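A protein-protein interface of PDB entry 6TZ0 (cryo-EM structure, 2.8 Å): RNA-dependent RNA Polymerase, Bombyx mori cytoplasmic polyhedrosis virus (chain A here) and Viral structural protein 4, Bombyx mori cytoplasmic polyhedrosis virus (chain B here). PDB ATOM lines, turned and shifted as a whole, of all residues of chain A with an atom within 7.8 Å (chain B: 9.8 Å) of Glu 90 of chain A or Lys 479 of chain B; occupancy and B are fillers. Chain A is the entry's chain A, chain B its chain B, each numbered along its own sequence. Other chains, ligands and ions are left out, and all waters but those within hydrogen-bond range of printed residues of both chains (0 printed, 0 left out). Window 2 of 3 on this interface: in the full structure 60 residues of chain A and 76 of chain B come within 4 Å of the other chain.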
ATOM      1  N   LEU A  88     -26.119 -24.243 -36.436  1.00  0.00           N
ATOM      2  CA  LEU A  88     -25.907 -23.411 -35.266  1.00  0.00           C
ATOM      3  C   LEU A  88     -25.267 -24.247 -34.168  1.00  0.00           C
ATOM      4  O   LEU A  88     -25.058 -25.453 -34.314  1.00  0.00           O
ATOM      5  CB  LEU A  88     -27.215 -22.798 -34.766  1.00  0.00           C
ATOM      6  CG  LEU A  88     -27.994 -21.881 -35.702  1.00  0.00           C
ATOM      7  CD1 LEU A  88     -29.197 -21.332 -34.976  1.00  0.00           C
ATOM      8  CD2 LEU A  88     -27.121 -20.776 -36.220  1.00  0.00           C
ATOM      9  N   ALA A  89     -24.962 -23.592 -33.057  1.00  0.00           N
ATOM     10  CA  ALA A  89     -24.487 -24.300 -31.883  1.00  0.00           C
ATOM     11  C   ALA A  89     -25.678 -24.756 -31.047  1.00  0.00           C
ATOM     12  O   ALA A  89     -26.837 -24.483 -31.371  1.00  0.00           O
ATOM     13  CB  ALA A  89     -23.539 -23.416 -31.080  1.00  0.00           C
ATOM     14  N   GLU A  90     -25.390 -25.476 -29.960  1.00  0.00           N
ATOM     15  CA  GLU A  90     -26.453 -25.947 -29.076  1.00  0.00           C
ATOM     16  C   GLU A  90     -27.115 -24.794 -28.342  1.00  0.00           C
ATOM     17  O   GLU A  90     -28.341 -24.761 -28.201  1.00  0.00           O
ATOM     18  CB  GLU A  90     -25.901 -26.964 -28.081  1.00  0.00           C
ATOM     19  CG  GLU A  90     -25.600 -28.323 -28.688  1.00  0.00           C
ATOM     20  CD  GLU A  90     -24.245 -28.395 -29.347  1.00  0.00           C
ATOM     21  OE1 GLU A  90     -23.487 -27.410 -29.263  1.00  0.00           O
ATOM     22  OE2 GLU A  90     -23.942 -29.442 -29.959  1.00  0.00           O
ATOM     23  N   ASP A  91     -26.324 -23.821 -27.901  1.00  0.00           N
ATOM     24  CA  ASP A  91     -26.872 -22.648 -27.239  1.00  0.00           C
ATOM     25  C   ASP A  91     -27.575 -21.725 -28.228  1.00  0.00           C
ATOM     26  O   ASP A  91     -28.370 -20.880 -27.806  1.00  0.00           O
ATOM     27  CB  ASP A  91     -25.738 -21.908 -26.526  1.00  0.00           C
ATOM     28  CG  ASP A  91     -26.220 -21.008 -25.409  1.00  0.00           C
ATOM     29  OD1 ASP A  91     -27.437 -20.969 -25.132  1.00  0.00           O
ATOM     30  OD2 ASP A  91     -25.370 -20.342 -24.785  1.00  0.00           O
ATOM     31  N   GLU A  92     -27.294 -21.887 -29.529  1.00  0.00           N
ATOM     32  CA  GLU A  92     -27.767 -21.019 -30.614  1.00  0.00           C
ATOM     33  C   GLU A  92     -27.392 -19.560 -30.381  1.00  0.00           C
ATOM     34  O   GLU A  92     -28.145 -18.649 -30.729  1.00  0.00           O
ATOM     35  CB  GLU A  92     -29.274 -21.168 -30.848  1.00  0.00           C
ATOM     36  CG  GLU A  92     -29.651 -22.515 -31.425  1.00  0.00           C
ATOM     37  CD  GLU A  92     -31.137 -22.674 -31.611  1.00  0.00           C
ATOM     38  OE1 GLU A  92     -31.890 -21.793 -31.149  1.00  0.00           O
ATOM     39  OE2 GLU A  92     -31.552 -23.678 -32.225  1.00  0.00           O
ATOM     40  N   SER A  93     -26.220 -19.342 -29.786  1.00  0.00           N
ATOM     41  CA  SER A  93     -25.715 -17.997 -29.563  1.00  0.00           C
ATOM     42  C   SER A  93     -24.984 -17.464 -30.781  1.00  0.00           C
ATOM     43  O   SER A  93     -24.890 -16.246 -30.957  1.00  0.00           O
ATOM     44  CB  SER A  93     -24.797 -17.987 -28.344  1.00  0.00           C
ATOM     45  OG  SER A  93     -23.685 -18.838 -28.536  1.00  0.00           O
ATOM     46  N   PHE A  94     -24.481 -18.358 -31.625  1.00  0.00           N
ATOM     47  CA  PHE A  94     -23.779 -18.011 -32.851  1.00  0.00           C
ATOM     48  C   PHE A  94     -23.838 -19.252 -33.739  1.00  0.00           C
ATOM     49  O   PHE A  94     -24.335 -20.300 -33.324  1.00  0.00           O
ATOM     50  CB  PHE A  94     -22.345 -17.544 -32.539  1.00  0.00           C
ATOM     51  CG  PHE A  94     -21.626 -16.928 -33.700  1.00  0.00           C
ATOM     52  CD1 PHE A  94     -22.006 -15.689 -34.184  1.00  0.00           C
ATOM     53  CD2 PHE A  94     -20.568 -17.584 -34.304  1.00  0.00           C
ATOM     54  CE1 PHE A  94     -21.352 -15.122 -35.255  1.00  0.00           C
ATOM     55  CE2 PHE A  94     -19.913 -17.023 -35.377  1.00  0.00           C
ATOM     56  CZ  PHE A  94     -20.305 -15.789 -35.850  1.00  0.00           C
ATOM     57  N   PHE A  95     -23.363 -19.116 -34.979  1.00  0.00           N
ATOM     58  CA  PHE A  95     -23.163 -20.259 -35.859  1.00  0.00           C
ATOM     59  C   PHE A  95     -22.175 -21.255 -35.262  1.00  0.00           C
ATOM     60  O   PHE A  95     -21.390 -20.938 -34.364  1.00  0.00           O
ATOM     61  CB  PHE A  95     -22.634 -19.823 -37.222  1.00  0.00           C
ATOM     62  CG  PHE A  95     -23.638 -19.120 -38.073  1.00  0.00           C
ATOM     63  CD1 PHE A  95     -24.616 -19.837 -38.740  1.00  0.00           C
ATOM     64  CD2 PHE A  95     -23.582 -17.749 -38.249  1.00  0.00           C
ATOM     65  CE1 PHE A  95     -25.542 -19.199 -39.537  1.00  0.00           C
ATOM     66  CE2 PHE A  95     -24.505 -17.105 -39.052  1.00  0.00           C
ATOM     67  CZ  PHE A  95     -25.484 -17.832 -39.696  1.00  0.00           C
ATOM     68  N   LYS A  96     -22.211 -22.472 -35.792  1.00  0.00           N
ATOM     69  CA  LYS A  96     -21.354 -23.545 -35.318  1.00  0.00           C
ATOM     70  C   LYS A  96     -19.896 -23.235 -35.652  1.00  0.00           C
ATOM     71  O   LYS A  96     -19.600 -22.498 -36.597  1.00  0.00           O
ATOM     72  CB  LYS A  96     -21.795 -24.874 -35.940  1.00  0.00           C
ATOM     73  CG  LYS A  96     -21.224 -26.127 -35.309  1.00  0.00           C
ATOM     74  CD  LYS A  96     -21.795 -27.374 -35.945  1.00  0.00           C
ATOM     75  CE  LYS A  96     -21.238 -28.616 -35.289  1.00  0.00           C
ATOM     76  NZ  LYS A  96     -21.803 -29.848 -35.890  1.00  0.00           N
ATOM     77  N   ILE B 345     -26.483 -12.741 -25.352  1.00  0.00           N
ATOM     78  CA  ILE B 345     -26.869 -14.106 -25.008  1.00  0.00           C
ATOM     79  C   ILE B 345     -25.958 -14.674 -23.929  1.00  0.00           C
ATOM     80  O   ILE B 345     -26.435 -15.192 -22.917  1.00  0.00           O
ATOM     81  CB  ILE B 345     -26.902 -14.998 -26.263  1.00  0.00           C
ATOM     82  CG1 ILE B 345     -28.021 -14.537 -27.194  1.00  0.00           C
ATOM     83  CG2 ILE B 345     -27.109 -16.450 -25.884  1.00  0.00           C
ATOM     84  CD1 ILE B 345     -28.032 -15.207 -28.532  1.00  0.00           C
ATOM     85  N   ASN B 346     -24.641 -14.576 -24.106  1.00  0.00           N
ATOM     86  CA  ASN B 346     -23.686 -15.069 -23.119  1.00  0.00           C
ATOM     87  C   ASN B 346     -22.724 -13.961 -22.720  1.00  0.00           C
ATOM     88  O   ASN B 346     -22.181 -13.267 -23.585  1.00  0.00           O
ATOM     89  CB  ASN B 346     -22.889 -16.259 -23.655  1.00  0.00           C
ATOM     90  CG  ASN B 346     -23.759 -17.434 -23.996  1.00  0.00           C
ATOM     91  OD1 ASN B 346     -23.794 -17.877 -25.139  1.00  0.00           O
ATOM     92  ND2 ASN B 346     -24.481 -17.942 -23.009  1.00  0.00           N
ATOM     93  N   PHE B 401     -18.657 -32.759 -22.365  1.00  0.00           N
ATOM     94  CA  PHE B 401     -18.407 -31.340 -22.151  1.00  0.00           C
ATOM     95  C   PHE B 401     -19.492 -30.718 -21.286  1.00  0.00           C
ATOM     96  O   PHE B 401     -19.720 -29.508 -21.361  1.00  0.00           O
ATOM     97  CB  PHE B 401     -18.315 -30.598 -23.486  1.00  0.00           C
ATOM     98  CG  PHE B 401     -17.120 -30.970 -24.315  1.00  0.00           C
ATOM     99  CD1 PHE B 401     -15.893 -30.360 -24.108  1.00  0.00           C
ATOM    100  CD2 PHE B 401     -17.225 -31.929 -25.309  1.00  0.00           C
ATOM    101  CE1 PHE B 401     -14.793 -30.704 -24.878  1.00  0.00           C
ATOM    102  CE2 PHE B 401     -16.130 -32.276 -26.080  1.00  0.00           C
ATOM    103  CZ  PHE B 401     -14.916 -31.663 -25.863  1.00  0.00           C
ATOM    104  N   ALA B 402     -20.182 -31.528 -20.489  1.00  0.00           N
ATOM    105  CA  ALA B 402     -21.257 -31.022 -19.651  1.00  0.00           C
ATOM    106  C   ALA B 402     -20.691 -30.193 -18.512  1.00  0.00           C
ATOM    107  O   ALA B 402     -19.616 -30.489 -17.989  1.00  0.00           O
ATOM    108  CB  ALA B 402     -22.086 -32.177 -19.099  1.00  0.00           C
ATOM    109  N   TYR B 403     -21.421 -29.140 -18.135  1.00  0.00           N
ATOM    110  CA  TYR B 403     -20.904 -28.181 -17.164  1.00  0.00           C
ATOM    111  C   TYR B 403     -20.787 -28.783 -15.770  1.00  0.00           C
ATOM    112  O   TYR B 403     -19.867 -28.441 -15.023  1.00  0.00           O
ATOM    113  CB  TYR B 403     -21.784 -26.932 -17.136  1.00  0.00           C
ATOM    114  CG  TYR B 403     -21.411 -25.969 -16.040  1.00  0.00           C
ATOM    115  CD1 TYR B 403     -20.253 -25.209 -16.117  1.00  0.00           C
ATOM    116  CD2 TYR B 403     -22.214 -25.827 -14.918  1.00  0.00           C
ATOM    117  CE1 TYR B 403     -19.908 -24.336 -15.106  1.00  0.00           C
ATOM    118  CE2 TYR B 403     -21.876 -24.963 -13.909  1.00  0.00           C
ATOM    119  CZ  TYR B 403     -20.725 -24.223 -14.004  1.00  0.00           C
ATOM    120  OH  TYR B 403     -20.397 -23.357 -12.991  1.00  0.00           O
ATOM    121  N   ASP B 404     -21.692 -29.692 -15.406  1.00  0.00           N
ATOM    122  CA  ASP B 404     -21.605 -30.300 -14.084  1.00  0.00           C
ATOM    123  C   ASP B 404     -20.458 -31.302 -13.992  1.00  0.00           C
ATOM    124  O   ASP B 404     -19.836 -31.425 -12.935  1.00  0.00           O
ATOM    125  CB  ASP B 404     -22.937 -30.948 -13.710  1.00  0.00           C
ATOM    126  CG  ASP B 404     -23.405 -31.984 -14.718  1.00  0.00           C
ATOM    127  OD1 ASP B 404     -22.790 -32.125 -15.796  1.00  0.00           O
ATOM    128  OD2 ASP B 404     -24.399 -32.677 -14.419  1.00  0.00           O
ATOM    129  N   ASN B 470     -11.689 -25.567 -28.419  1.00  0.00           N
ATOM    130  CA  ASN B 470     -12.923 -26.338 -28.498  1.00  0.00           C
ATOM    131  C   ASN B 470     -13.487 -26.654 -27.122  1.00  0.00           C
ATOM    132  O   ASN B 470     -14.704 -26.778 -26.978  1.00  0.00           O
ATOM    133  CB  ASN B 470     -12.689 -27.645 -29.238  1.00  0.00           C
ATOM    134  CG  ASN B 470     -13.976 -28.314 -29.654  1.00  0.00           C
ATOM    135  OD1 ASN B 470     -15.035 -27.703 -29.655  1.00  0.00           O
ATOM    136  ND2 ASN B 470     -13.899 -29.599 -29.939  1.00  0.00           N
ATOM    137  N   TYR B 473     -15.268 -23.629 -26.110  1.00  0.00           N
ATOM    138  CA  TYR B 473     -16.424 -23.508 -26.994  1.00  0.00           C
ATOM    139  C   TYR B 473     -17.562 -24.428 -26.566  1.00  0.00           C
ATOM    140  O   TYR B 473     -18.718 -24.003 -26.483  1.00  0.00           O
ATOM    141  CB  TYR B 473     -16.009 -23.819 -28.429  1.00  0.00           C
ATOM    142  CG  TYR B 473     -17.148 -23.817 -29.417  1.00  0.00           C
ATOM    143  CD1 TYR B 473     -17.697 -22.628 -29.869  1.00  0.00           C
ATOM    144  CD2 TYR B 473     -17.670 -25.009 -29.899  1.00  0.00           C
ATOM    145  CE1 TYR B 473     -18.737 -22.626 -30.775  1.00  0.00           C
ATOM    146  CE2 TYR B 473     -18.705 -25.017 -30.800  1.00  0.00           C
ATOM    147  CZ  TYR B 473     -19.234 -23.826 -31.234  1.00  0.00           C
ATOM    148  OH  TYR B 473     -20.267 -23.841 -32.137  1.00  0.00           O
ATOM    149  N   MET B 474     -17.259 -25.698 -26.315  1.00  0.00           N
ATOM    150  CA  MET B 474     -18.286 -26.665 -25.964  1.00  0.00           C
ATOM    151  C   MET B 474     -18.755 -26.534 -24.525  1.00  0.00           C
ATOM    152  O   MET B 474     -19.805 -27.081 -24.182  1.00  0.00           O
ATOM    153  CB  MET B 474     -17.784 -28.088 -26.206  1.00  0.00           C
ATOM    154  CG  MET B 474     -17.552 -28.452 -27.656  1.00  0.00           C
ATOM    155  SD  MET B 474     -19.040 -28.405 -28.660  1.00  0.00           S
ATOM    156  CE  MET B 474     -19.914 -29.821 -28.010  1.00  0.00           C
ATOM    157  N   VAL B 475     -18.003 -25.845 -23.671  1.00  0.00           N
ATOM    158  CA  VAL B 475     -18.538 -25.527 -22.352  1.00  0.00           C
ATOM    159  C   VAL B 475     -19.377 -24.255 -22.404  1.00  0.00           C
ATOM    160  O   VAL B 475     -20.463 -24.197 -21.821  1.00  0.00           O
ATOM    161  CB  VAL B 475     -17.399 -25.432 -21.319  1.00  0.00           C
ATOM    162  CG1 VAL B 475     -17.907 -24.911 -19.995  1.00  0.00           C
ATOM    163  CG2 VAL B 475     -16.786 -26.794 -21.103  1.00  0.00           C
ATOM    164  N   SER B 476     -18.925 -23.241 -23.146  1.00  0.00           N
ATOM    165  CA  SER B 476     -19.611 -21.954 -23.144  1.00  0.00           C
ATOM    166  C   SER B 476     -20.934 -21.999 -23.899  1.00  0.00           C
ATOM    167  O   SER B 476     -21.888 -21.320 -23.510  1.00  0.00           O
ATOM    168  CB  SER B 476     -18.709 -20.887 -23.753  1.00  0.00           C
ATOM    169  OG  SER B 476     -17.516 -20.777 -23.011  1.00  0.00           O
ATOM    170  N   THR B 477     -21.010 -22.773 -24.979  1.00  0.00           N
ATOM    171  CA  THR B 477     -22.217 -22.845 -25.790  1.00  0.00           C
ATOM    172  C   THR B 477     -23.013 -24.116 -25.527  1.00  0.00           C
ATOM    173  O   THR B 477     -23.681 -24.625 -26.429  1.00  0.00           O
ATOM    174  CB  THR B 477     -21.878 -22.730 -27.275  1.00  0.00           C
ATOM    175  OG1 THR B 477     -21.020 -23.810 -27.660  1.00  0.00           O
ATOM    176  CG2 THR B 477     -21.187 -21.415 -27.564  1.00  0.00           C
ATOM    177  N   GLY B 478     -22.963 -24.633 -24.306  1.00  0.00           N
ATOM    178  CA  GLY B 478     -23.740 -25.795 -23.945  1.00  0.00           C
ATOM    179  C   GLY B 478     -25.192 -25.460 -23.677  1.00  0.00           C
ATOM    180  O   GLY B 478     -25.626 -24.311 -23.729  1.00  0.00           O
ATOM    181  N   LYS B 479     -25.963 -26.511 -23.393  1.00  0.00           N
ATOM    182  CA  LYS B 479     -27.371 -26.349 -23.042  1.00  0.00           C
ATOM    183  C   LYS B 479     -27.541 -25.970 -21.578  1.00  0.00           C
ATOM    184  O   LYS B 479     -28.216 -24.988 -21.256  1.00  0.00           O
ATOM    185  CB  LYS B 479     -28.138 -27.639 -23.335  1.00  0.00           C
ATOM    186  CG  LYS B 479     -28.261 -28.013 -24.797  1.00  0.00           C
ATOM    187  CD  LYS B 479     -29.276 -27.141 -25.507  1.00  0.00           C
ATOM    188  CE  LYS B 479     -29.428 -27.567 -26.952  1.00  0.00           C
ATOM    189  NZ  LYS B 479     -30.032 -28.914 -27.074  1.00  0.00           N
ATOM    190  N   THR B 480     -26.943 -26.743 -20.676  1.00  0.00           N
ATOM    191  CA  THR B 480     -27.156 -26.584 -19.247  1.00  0.00           C
ATOM    192  C   THR B 480     -26.131 -25.669 -18.596  1.00  0.00           C
ATOM    193  O   THR B 480     -26.118 -25.547 -17.367  1.00  0.00           O
ATOM    194  CB  THR B 480     -27.136 -27.946 -18.559  1.00  0.00           C
ATOM    195  OG1 THR B 480     -25.821 -28.502 -18.647  1.00  0.00           O
ATOM    196  CG2 THR B 480     -28.097 -28.881 -19.250  1.00  0.00           C
ATOM    197  N   THR B 481     -25.270 -25.038 -19.379  1.00  0.00           N
ATOM    198  CA  THR B 481     -24.299 -24.134 -18.794  1.00  0.00           C
ATOM    199  C   THR B 481     -24.966 -22.801 -18.448  1.00  0.00           C
ATOM    200  O   THR B 481     -25.933 -22.396 -19.099  1.00  0.00           O
ATOM    201  CB  THR B 481     -23.119 -23.934 -19.751  1.00  0.00           C
ATOM    202  OG1 THR B 481     -22.117 -23.117 -19.139  1.00  0.00           O
ATOM    203  CG2 THR B 481     -23.554 -23.321 -21.070  1.00  0.00           C
ATOM    204  N   PRO B 482     -24.530 -22.147 -17.374  1.00  0.00           N
ATOM    205  CA  PRO B 482     -25.147 -20.876 -16.991  1.00  0.00           C
ATOM    206  C   PRO B 482     -24.817 -19.764 -17.972  1.00  0.00           C
ATOM    207  O   PRO B 482     -23.869 -19.840 -18.754  1.00  0.00           O
ATOM    208  CB  PRO B 482     -24.553 -20.595 -15.611  1.00  0.00           C
ATOM    209  CG  PRO B 482     -24.176 -21.909 -15.102  1.00  0.00           C
ATOM    210  CD  PRO B 482     -23.707 -22.687 -16.280  1.00  0.00           C
ATOM    211  N   ARG B 483     -25.643 -18.722 -17.923  1.00  0.00           N
ATOM    212  CA  ARG B 483     -25.529 -17.626 -18.878  1.00  0.00           C
ATOM    213  C   ARG B 483     -24.286 -16.782 -18.618  1.00  0.00           C
ATOM    214  O   ARG B 483     -23.562 -16.420 -19.552  1.00  0.00           O
ATOM    215  CB  ARG B 483     -26.785 -16.761 -18.818  1.00  0.00           C
ATOM    216  CG  ARG B 483     -26.707 -15.560 -19.702  1.00  0.00           C
ATOM    217  CD  ARG B 483     -27.913 -14.680 -19.603  1.00  0.00           C
ATOM    218  NE  ARG B 483     -27.726 -13.495 -20.425  1.00  0.00           N
ATOM    219  CZ  ARG B 483     -27.168 -12.374 -19.985  1.00  0.00           C
ATOM    220  NH1 ARG B 483     -26.762 -12.288 -18.730  1.00  0.00           N
ATOM    221  NH2 ARG B 483     -27.030 -11.338 -20.793  1.00  0.00           N
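OD1 of Asn 346 of chain B lies close to OD2 of Asp 91 of chain A. N of Asp 91 of chain A lies within hydrogen-bond range of O of Thr 477 of chain B (3.1 Å).
The backbone NH of Ala 89 of chain A lies within hydrogen-bond range of the backbone carbonyl oxygen of Phe 94 of chain A. O of Ile 345 of chain B lies close to NE of Arg 483 of chain B (3.3 Å). O of Tyr 473 of chain B sits at hydrogen-bond distance from OG1 of Thr 477 of chain B (2.6 Å).
Ala 89 of chain A touches Tyr 473 of chain B (CB to OH, 3.5 Å). Thr 477 of chain B touches Glu 90 of chain A. Glu 90 of chain A touches Lys 479 of chain B. Ser 476 of chain B touches Asp 91 of chain A. O of Gly 478 of chain B touches CB of Asp 91 of chain A, at 3.7 Å. Ser 93 of chain A touches Ile 345 of chain B. Ser 93 of chain A touches Asn 346 of chain B (CB to OD1, 3.4 Å). OG of Ser 93 of chain A touches CG2 of Thr 477 of chain B, 3.7 Å away. Phe 95 of chain A touches Tyr 473 of chain B. Lys 96 of chain A touches Tyr 473 of chain B.
Glu 90 of chain A touches just these residues of chain B: Thr 477 (3.6 Å) and Lys 479 (3.3 Å). Gly 478 of chain B touches one residue of chain A. Printed residues of chain B within 4 Å of Ser 93 of chain A: Ile 345 (3.7 Å), Asn 346 (3.4 Å) and Thr 477 (3.7 Å). Printed residues of chain A within 4 Å of Ile 345 of chain B: Ser 93 (3.7 Å). Of the printed residues of chain B, Lys 96 of chain A touches Tyr 473. Of the printed residues of chain B, Phe 95 of chain A touches Tyr 473 (3.8 Å). Printed residues of chain B within 4 Å of Asp 91 of chain A: Asn 346, Ser 476, Thr 477 and Gly 478. The nearest residue of chain B that does not touch Glu 90 of chain A is Met 474 of chain B (4.5 Å). The nearest printed residue of chain B that does not touch Ser 93 of chain A is Ser 476 of chain B (5.9 Å).
Of the 18 printed residues of chain B, 7 touch a printed residue of chain A. Hydrophobic or aromatic side chains of chain B within 4 Å of the printed part of chain A: Ile 345 and Tyr 473. Of the 9 printed residues of chain A, 6 touch a printed residue of chain B. Printed residues of chain A that touch a printed residue of chain B: Ala 89, Glu 90, Asp 91, Ser 93, Phe 95 and Lys 96. Hydrophobic or aromatic side chains of chain A that line the printed part of chain B: Ala 89. Among the printed residues, 12 pairs touch across the chains.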
